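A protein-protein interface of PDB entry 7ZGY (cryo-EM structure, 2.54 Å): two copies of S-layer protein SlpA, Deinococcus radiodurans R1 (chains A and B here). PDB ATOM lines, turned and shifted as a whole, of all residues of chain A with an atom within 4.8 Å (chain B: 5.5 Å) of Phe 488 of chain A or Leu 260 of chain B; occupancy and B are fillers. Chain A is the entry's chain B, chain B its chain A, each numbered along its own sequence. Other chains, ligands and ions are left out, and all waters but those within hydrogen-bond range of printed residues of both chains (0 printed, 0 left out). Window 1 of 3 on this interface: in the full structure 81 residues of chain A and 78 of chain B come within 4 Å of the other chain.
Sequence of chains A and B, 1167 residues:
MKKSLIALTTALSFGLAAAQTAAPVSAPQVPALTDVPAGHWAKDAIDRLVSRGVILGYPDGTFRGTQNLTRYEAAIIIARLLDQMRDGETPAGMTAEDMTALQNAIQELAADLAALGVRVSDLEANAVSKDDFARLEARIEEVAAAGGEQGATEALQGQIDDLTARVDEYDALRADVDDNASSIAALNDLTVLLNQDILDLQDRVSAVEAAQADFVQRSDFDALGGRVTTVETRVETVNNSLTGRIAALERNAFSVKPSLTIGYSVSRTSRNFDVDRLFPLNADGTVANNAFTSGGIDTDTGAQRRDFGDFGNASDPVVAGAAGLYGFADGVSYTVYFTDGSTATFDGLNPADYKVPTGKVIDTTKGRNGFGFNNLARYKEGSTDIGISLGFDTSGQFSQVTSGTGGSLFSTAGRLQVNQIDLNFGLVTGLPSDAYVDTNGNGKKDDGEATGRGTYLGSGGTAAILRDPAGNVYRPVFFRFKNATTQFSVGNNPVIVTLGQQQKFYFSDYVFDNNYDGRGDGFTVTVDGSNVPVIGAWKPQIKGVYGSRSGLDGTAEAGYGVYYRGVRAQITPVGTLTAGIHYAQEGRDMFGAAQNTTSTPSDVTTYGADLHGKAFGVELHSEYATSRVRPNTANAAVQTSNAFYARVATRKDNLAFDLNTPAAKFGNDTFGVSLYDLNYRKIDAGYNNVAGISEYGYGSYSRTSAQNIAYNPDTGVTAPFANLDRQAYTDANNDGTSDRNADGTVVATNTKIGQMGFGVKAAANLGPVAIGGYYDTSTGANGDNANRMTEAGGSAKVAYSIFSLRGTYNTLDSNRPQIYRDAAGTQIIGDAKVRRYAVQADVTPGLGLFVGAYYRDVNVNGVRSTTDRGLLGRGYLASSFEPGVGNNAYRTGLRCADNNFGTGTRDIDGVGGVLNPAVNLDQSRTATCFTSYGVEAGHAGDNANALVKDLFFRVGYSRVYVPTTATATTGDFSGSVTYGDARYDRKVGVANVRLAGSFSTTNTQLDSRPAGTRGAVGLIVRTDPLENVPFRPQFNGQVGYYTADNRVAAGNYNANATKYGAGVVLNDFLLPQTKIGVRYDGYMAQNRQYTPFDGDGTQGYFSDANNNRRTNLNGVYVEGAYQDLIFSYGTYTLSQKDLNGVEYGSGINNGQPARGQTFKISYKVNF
OD1 of Asn 419 of chain A lies within hydrogen-bond range of OH of Tyr 1163 of chain B.
The backbone carbonyl oxygen (O) of Val 497 of chain A sits at hydrogen-bond distance from the backbone NH (N) of Val 490 of chain A. N of Leu 499 of chain A lies within hydrogen-bond range of O of Phe 488 of chain A, 2.9 Å away. The side-chain amide nitrogen (ND2) of Asn 419 of chain A sits at hydrogen-bond distance from the backbone carbonyl oxygen (O) of Ser 489 of chain A (3.1 Å). The backbone NH (N) of Asn 419 of chain A sits at hydrogen-bond distance from the backbone carbonyl oxygen (O) of Val 401 of chain A, 2.9 Å away.
Among the printed residues, pairs that only touch across the chains: Val 401 of chain A with Val 1165 of chain B (3.9 Å), Val 401 of chain A with Phe 1167 of chain B (3.9 Å), Ile 421 of chain A with Phe 1167 of chain B (3.3 Å), Phe 488 of chain A with Leu 260 of chain B (3.5 Å), Phe 488 of chain A with Ile 262 of chain B (3.6 Å) and Val 490 of chain A with Tyr 1163 of chain B (3.6 Å).
Of the printed residues of chain B, Phe 488 of chain A touches Leu 260 (3.5 Å) and Ile 262 (3.6 Å). Leu 260 of chain B touches just one residue of chain A: Phe 488. Of the printed residues of chain A, Val 1165 of chain B touches Val 401 (3.9 Å). Printed residues of chain B within 4 Å of Asn 419 of chain A: Tyr 1163. Of the printed residues of chain A, Phe 1167 of chain B touches Val 401 and Ile 421. Thr 485 of chain A touches none of the printed residues of chain B. Ser 489 of chain A touches none of the printed residues of chain B. The nearest residue of chain A that does not touch Leu 260 of chain B is Ile 421 of chain A (4.4 Å).
Hydrophobic or aromatic side chains of chain A within 4 Å of the printed part of chain B: Val 401, Ile 421, Phe 488 and Val 490. Printed residues of chain B that touch a printed residue of chain A: Leu 260, Ile 262, Tyr 1163, Val 1165 and Phe 1167. Hydrophobic or aromatic side chains of chain B within 4 Å of the printed part of chain A: Leu 260, Ile 262, Tyr 1163, Val 1165 and Phe 1167. Among the printed residues, no Asp or Glu carboxylate lies within 4 Å of a Lys or Arg side-chain nitrogen of the other chain.
No position is printed for both chains. Of the 7 pairs that touch across the chains among the printed residues, none has its exchanged pair printed and touching as well.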
ATOM      1  N   VAL A 401     -28.082  36.004 -23.834  1.00  0.00           N
ATOM      2  CA  VAL A 401     -26.782  35.993 -23.177  1.00  0.00           C
ATOM      3  C   VAL A 401     -25.764  36.622 -24.116  1.00  0.00           C
ATOM      4  O   VAL A 401     -25.829  36.432 -25.334  1.00  0.00           O
ATOM      5  CB  VAL A 401     -26.342  34.570 -22.775  1.00  0.00           C
ATOM      6  CG1 VAL A 401     -27.170  34.065 -21.608  1.00  0.00           C
ATOM      7  CG2 VAL A 401     -26.439  33.625 -23.956  1.00  0.00           C
ATOM      8  N   ASN A 419     -26.507  35.252 -27.870  1.00  0.00           N
ATOM      9  CA  ASN A 419     -27.157  33.962 -28.017  1.00  0.00           C
ATOM     10  C   ASN A 419     -28.532  33.996 -27.368  1.00  0.00           C
ATOM     11  O   ASN A 419     -28.684  34.466 -26.237  1.00  0.00           O
ATOM     12  CB  ASN A 419     -26.311  32.851 -27.390  1.00  0.00           C
ATOM     13  CG  ASN A 419     -25.194  32.388 -28.298  1.00  0.00           C
ATOM     14  OD1 ASN A 419     -24.022  32.439 -27.934  1.00  0.00           O
ATOM     15  ND2 ASN A 419     -25.555  31.920 -29.483  1.00  0.00           N
ATOM     16  N   ILE A 421     -31.401  32.075 -25.609  1.00  0.00           N
ATOM     17  CA  ILE A 421     -31.582  30.863 -24.830  1.00  0.00           C
ATOM     18  C   ILE A 421     -33.072  30.658 -24.576  1.00  0.00           C
ATOM     19  O   ILE A 421     -33.899  31.533 -24.829  1.00  0.00           O
ATOM     20  CB  ILE A 421     -30.786  30.896 -23.514  1.00  0.00           C
ATOM     21  CG1 ILE A 421     -31.396  31.901 -22.540  1.00  0.00           C
ATOM     22  CG2 ILE A 421     -29.330  31.234 -23.786  1.00  0.00           C
ATOM     23  CD1 ILE A 421     -30.913  31.735 -21.126  1.00  0.00           C
ATOM     24  N   THR A 485     -32.315  24.937 -24.276  1.00  0.00           N
ATOM     25  CA  THR A 485     -31.194  25.281 -25.136  1.00  0.00           C
ATOM     26  C   THR A 485     -29.968  24.472 -24.740  1.00  0.00           C
ATOM     27  O   THR A 485     -29.569  24.465 -23.572  1.00  0.00           O
ATOM     28  CB  THR A 485     -30.885  26.776 -25.052  1.00  0.00           C
ATOM     29  OG1 THR A 485     -32.008  27.524 -25.534  1.00  0.00           O
ATOM     30  CG2 THR A 485     -29.665  27.114 -25.887  1.00  0.00           C
ATOM     31  N   THR A 486     -29.372  23.792 -25.720  1.00  0.00           N
ATOM     32  CA  THR A 486     -28.148  23.034 -25.503  1.00  0.00           C
ATOM     33  C   THR A 486     -27.088  23.337 -26.553  1.00  0.00           C
ATOM     34  O   THR A 486     -25.986  22.785 -26.476  1.00  0.00           O
ATOM     35  CB  THR A 486     -28.436  21.528 -25.481  1.00  0.00           C
ATOM     36  OG1 THR A 486     -29.295  21.187 -26.575  1.00  0.00           O
ATOM     37  CG2 THR A 486     -29.108  21.136 -24.177  1.00  0.00           C
ATOM     38  N   GLN A 487     -27.386  24.200 -27.521  1.00  0.00           N
ATOM     39  CA  GLN A 487     -26.461  24.533 -28.594  1.00  0.00           C
ATOM     40  C   GLN A 487     -26.210  26.032 -28.589  1.00  0.00           C
ATOM     41  O   GLN A 487     -27.149  26.819 -28.433  1.00  0.00           O
ATOM     42  CB  GLN A 487     -27.012  24.099 -29.955  1.00  0.00           C
ATOM     43  CG  GLN A 487     -27.692  22.740 -29.959  1.00  0.00           C
ATOM     44  CD  GLN A 487     -26.712  21.591 -30.038  1.00  0.00           C
ATOM     45  OE1 GLN A 487     -25.940  21.488 -30.988  1.00  0.00           O
ATOM     46  NE2 GLN A 487     -26.748  20.713 -29.046  1.00  0.00           N
ATOM     47  N   PHE A 488     -24.951  26.424 -28.760  1.00  0.00           N
ATOM     48  CA  PHE A 488     -24.560  27.825 -28.810  1.00  0.00           C
ATOM     49  C   PHE A 488     -23.725  28.057 -30.059  1.00  0.00           C
ATOM     50  O   PHE A 488     -22.749  27.340 -30.292  1.00  0.00           O
ATOM     51  CB  PHE A 488     -23.777  28.225 -27.557  1.00  0.00           C
ATOM     52  CG  PHE A 488     -24.585  28.160 -26.296  1.00  0.00           C
ATOM     53  CD1 PHE A 488     -24.819  26.949 -25.670  1.00  0.00           C
ATOM     54  CD2 PHE A 488     -25.113  29.308 -25.738  1.00  0.00           C
ATOM     55  CE1 PHE A 488     -25.567  26.885 -24.515  1.00  0.00           C
ATOM     56  CE2 PHE A 488     -25.859  29.249 -24.583  1.00  0.00           C
ATOM     57  CZ  PHE A 488     -26.086  28.035 -23.971  1.00  0.00           C
ATOM     58  N   SER A 489     -24.101  29.060 -30.847  1.00  0.00           N
ATOM     59  CA  SER A 489     -23.474  29.333 -32.132  1.00  0.00           C
ATOM     60  C   SER A 489     -22.730  30.660 -32.086  1.00  0.00           C
ATOM     61  O   SER A 489     -23.197  31.623 -31.472  1.00  0.00           O
ATOM     62  CB  SER A 489     -24.516  29.361 -33.251  1.00  0.00           C
ATOM     63  OG  SER A 489     -25.223  28.138 -33.313  1.00  0.00           O
ATOM     64  N   VAL A 490     -21.571  30.703 -32.738  1.00  0.00           N
ATOM     65  CA  VAL A 490     -20.745  31.901 -32.814  1.00  0.00           C
ATOM     66  C   VAL A 490     -20.276  32.087 -34.249  1.00  0.00           C
ATOM     67  O   VAL A 490     -19.938  31.113 -34.932  1.00  0.00           O
ATOM     68  CB  VAL A 490     -19.538  31.827 -31.854  1.00  0.00           C
ATOM     69  CG1 VAL A 490     -19.993  31.445 -30.460  1.00  0.00           C
ATOM     70  CG2 VAL A 490     -18.510  30.850 -32.370  1.00  0.00           C
ATOM     71  N   VAL A 497     -19.716  28.327 -35.725  1.00  0.00           N
ATOM     72  CA  VAL A 497     -19.288  27.232 -34.863  1.00  0.00           C
ATOM     73  C   VAL A 497     -20.343  27.027 -33.788  1.00  0.00           C
ATOM     74  O   VAL A 497     -20.690  27.968 -33.066  1.00  0.00           O
ATOM     75  CB  VAL A 497     -17.913  27.513 -34.233  1.00  0.00           C
ATOM     76  CG1 VAL A 497     -17.391  26.273 -33.539  1.00  0.00           C
ATOM     77  CG2 VAL A 497     -16.936  27.983 -35.287  1.00  0.00           C
ATOM     78  N   THR A 498     -20.850  25.803 -33.681  1.00  0.00           N
ATOM     79  CA  THR A 498     -21.905  25.451 -32.739  1.00  0.00           C
ATOM     80  C   THR A 498     -21.360  24.438 -31.747  1.00  0.00           C
ATOM     81  O   THR A 498     -20.882  23.371 -32.145  1.00  0.00           O
ATOM     82  CB  THR A 498     -23.122  24.880 -33.468  1.00  0.00           C
ATOM     83  OG1 THR A 498     -23.585  25.819 -34.444  1.00  0.00           O
ATOM     84  CG2 THR A 498     -24.240  24.585 -32.485  1.00  0.00           C
ATOM     85  N   LEU A 499     -21.439  24.768 -30.464  1.00  0.00           N
ATOM     86  CA  LEU A 499     -20.992  23.905 -29.382  1.00  0.00           C
ATOM     87  C   LEU A 499     -22.193  23.461 -28.562  1.00  0.00           C
ATOM     88  O   LEU A 499     -23.067  24.272 -28.247  1.00  0.00           O
ATOM     89  CB  LEU A 499     -19.992  24.633 -28.479  1.00  0.00           C
ATOM     90  CG  LEU A 499     -19.632  23.974 -27.145  1.00  0.00           C
ATOM     91  CD1 LEU A 499     -18.798  22.723 -27.349  1.00  0.00           C
ATOM     92  CD2 LEU A 499     -18.923  24.954 -26.229  1.00  0.00           C
ATOM     93  N   PRO B 258     -29.269  35.484 -12.922  1.00  0.00           N
ATOM     94  CA  PRO B 258     -29.037  34.134 -13.430  1.00  0.00           C
ATOM     95  C   PRO B 258     -27.651  33.993 -14.037  1.00  0.00           C
ATOM     96  O   PRO B 258     -27.066  34.941 -14.566  1.00  0.00           O
ATOM     97  CB  PRO B 258     -30.127  33.972 -14.500  1.00  0.00           C
ATOM     98  CG  PRO B 258     -30.585  35.374 -14.836  1.00  0.00           C
ATOM     99  CD  PRO B 258     -29.880  36.351 -13.940  1.00  0.00           C
ATOM    100  N   SER B 259     -27.127  32.778 -13.949  1.00  0.00           N
ATOM    101  CA  SER B 259     -25.797  32.459 -14.441  1.00  0.00           C
ATOM    102  C   SER B 259     -25.859  31.188 -15.269  1.00  0.00           C
ATOM    103  O   SER B 259     -26.527  30.222 -14.891  1.00  0.00           O
ATOM    104  CB  SER B 259     -24.804  32.284 -13.286  1.00  0.00           C
ATOM    105  OG  SER B 259     -24.665  33.479 -12.541  1.00  0.00           O
ATOM    106  N   LEU B 260     -25.154  31.196 -16.397  1.00  0.00           N
ATOM    107  CA  LEU B 260     -25.056  30.048 -17.285  1.00  0.00           C
ATOM    108  C   LEU B 260     -23.595  29.821 -17.635  1.00  0.00           C
ATOM    109  O   LEU B 260     -22.893  30.761 -18.019  1.00  0.00           O
ATOM    110  CB  LEU B 260     -25.883  30.260 -18.555  1.00  0.00           C
ATOM    111  CG  LEU B 260     -25.859  29.139 -19.593  1.00  0.00           C
ATOM    112  CD1 LEU B 260     -26.657  27.947 -19.108  1.00  0.00           C
ATOM    113  CD2 LEU B 260     -26.405  29.645 -20.909  1.00  0.00           C
ATOM    114  N   THR B 261     -23.142  28.581 -17.493  1.00  0.00           N
ATOM    115  CA  THR B 261     -21.788  28.187 -17.855  1.00  0.00           C
ATOM    116  C   THR B 261     -21.864  27.115 -18.928  1.00  0.00           C
ATOM    117  O   THR B 261     -22.565  26.115 -18.759  1.00  0.00           O
ATOM    118  CB  THR B 261     -21.008  27.661 -16.647  1.00  0.00           C
ATOM    119  OG1 THR B 261     -21.459  26.340 -16.327  1.00  0.00           O
ATOM    120  CG2 THR B 261     -21.209  28.564 -15.445  1.00  0.00           C
ATOM    121  N   ILE B 262     -21.149  27.325 -20.026  1.00  0.00           N
ATOM    122  CA  ILE B 262     -21.092  26.389 -21.141  1.00  0.00           C
ATOM    123  C   ILE B 262     -19.641  26.008 -21.382  1.00  0.00           C
ATOM    124  O   ILE B 262     -18.769  26.881 -21.458  1.00  0.00           O
ATOM    125  CB  ILE B 262     -21.731  26.986 -22.411  1.00  0.00           C
ATOM    126  CG1 ILE B 262     -21.934  25.908 -23.477  1.00  0.00           C
ATOM    127  CG2 ILE B 262     -20.921  28.157 -22.929  1.00  0.00           C
ATOM    128  CD1 ILE B 262     -22.923  24.857 -23.102  1.00  0.00           C
ATOM    129  N   ILE B 386     -23.457  22.241 -19.316  1.00  0.00           N
ATOM    130  CA  ILE B 386     -24.208  23.470 -19.095  1.00  0.00           C
ATOM    131  C   ILE B 386     -24.582  23.522 -17.622  1.00  0.00           C
ATOM    132  O   ILE B 386     -25.226  22.604 -17.103  1.00  0.00           O
ATOM    133  CB  ILE B 386     -25.469  23.553 -19.972  1.00  0.00           C
ATOM    134  CG1 ILE B 386     -25.125  23.580 -21.458  1.00  0.00           C
ATOM    135  CG2 ILE B 386     -26.270  24.782 -19.616  1.00  0.00           C
ATOM    136  CD1 ILE B 386     -25.021  22.236 -22.095  1.00  0.00           C
ATOM    137  N   GLY B 387     -24.181  24.593 -16.951  1.00  0.00           N
ATOM    138  CA  GLY B 387     -24.547  24.800 -15.567  1.00  0.00           C
ATOM    139  C   GLY B 387     -25.406  26.033 -15.407  1.00  0.00           C
ATOM    140  O   GLY B 387     -25.034  27.108 -15.880  1.00  0.00           O
ATOM    141  N   ILE B 388     -26.552  25.893 -14.749  1.00  0.00           N
ATOM    142  CA  ILE B 388     -27.511  26.978 -14.585  1.00  0.00           C
ATOM    143  C   ILE B 388     -27.661  27.271 -13.101  1.00  0.00           C
ATOM    144  O   ILE B 388     -27.827  26.350 -12.295  1.00  0.00           O
ATOM    145  CB  ILE B 388     -28.872  26.630 -15.215  1.00  0.00           C
ATOM    146  CG1 ILE B 388     -28.752  26.583 -16.739  1.00  0.00           C
ATOM    147  CG2 ILE B 388     -29.931  27.631 -14.790  1.00  0.00           C
ATOM    148  CD1 ILE B 388     -29.967  26.023 -17.429  1.00  0.00           C
ATOM    149  N   SER B 389     -27.598  28.551 -12.744  1.00  0.00           N
ATOM    150  CA  SER B 389     -27.765  28.972 -11.363  1.00  0.00           C
ATOM    151  C   SER B 389     -28.588  30.248 -11.330  1.00  0.00           C
ATOM    152  O   SER B 389     -28.675  30.978 -12.317  1.00  0.00           O
ATOM    153  CB  SER B 389     -26.416  29.196 -10.674  1.00  0.00           C
ATOM    154  OG  SER B 389     -25.731  30.289 -11.257  1.00  0.00           O
ATOM    155  N   TYR B1163     -16.458  29.109 -23.338  1.00  0.00           N
ATOM    156  CA  TYR B1163     -17.370  30.137 -23.825  1.00  0.00           C
ATOM    157  C   TYR B1163     -18.001  30.808 -22.614  1.00  0.00           C
ATOM    158  O   TYR B1163     -18.819  30.194 -21.925  1.00  0.00           O
ATOM    159  CB  TYR B1163     -18.434  29.532 -24.735  1.00  0.00           C
ATOM    160  CG  TYR B1163     -19.236  30.539 -25.523  1.00  0.00           C
ATOM    161  CD1 TYR B1163     -18.612  31.529 -26.264  1.00  0.00           C
ATOM    162  CD2 TYR B1163     -20.619  30.491 -25.531  1.00  0.00           C
ATOM    163  CE1 TYR B1163     -19.345  32.444 -26.987  1.00  0.00           C
ATOM    164  CE2 TYR B1163     -21.359  31.399 -26.250  1.00  0.00           C
ATOM    165  CZ  TYR B1163     -20.719  32.374 -26.976  1.00  0.00           C
ATOM    166  OH  TYR B1163     -21.464  33.280 -27.692  1.00  0.00           O
ATOM    167  N   VAL B1165     -20.489  33.493 -21.032  1.00  0.00           N
ATOM    168  CA  VAL B1165     -21.728  34.163 -21.393  1.00  0.00           C
ATOM    169  C   VAL B1165     -22.302  34.838 -20.157  1.00  0.00           C
ATOM    170  O   VAL B1165     -22.195  34.326 -19.039  1.00  0.00           O
ATOM    171  CB  VAL B1165     -22.755  33.187 -22.004  1.00  0.00           C
ATOM    172  CG1 VAL B1165     -22.298  32.729 -23.372  1.00  0.00           C
ATOM    173  CG2 VAL B1165     -22.961  31.998 -21.088  1.00  0.00           C
ATOM    174  N   PHE B1167     -25.772  37.253 -18.604  1.00  0.00           N
ATOM    175  CA  PHE B1167     -27.169  37.610 -18.790  1.00  0.00           C
ATOM    176  C   PHE B1167     -27.339  39.124 -18.834  1.00  0.00           C
ATOM    177  O   PHE B1167     -27.157  39.747 -19.879  1.00  0.00           O
ATOM    178  CB  PHE B1167     -28.032  37.016 -17.678  1.00  0.00           C
ATOM    179  CG  PHE B1167     -28.546  35.641 -17.979  1.00  0.00           C
ATOM    180  CD1 PHE B1167     -27.798  34.524 -17.660  1.00  0.00           C
ATOM    181  CD2 PHE B1167     -29.774  35.465 -18.587  1.00  0.00           C
ATOM    182  CE1 PHE B1167     -28.266  33.258 -17.937  1.00  0.00           C
ATOM    183  CE2 PHE B1167     -30.246  34.201 -18.866  1.00  0.00           C
ATOM    184  CZ  PHE B1167     -29.492  33.097 -18.539  1.00  0.00           C
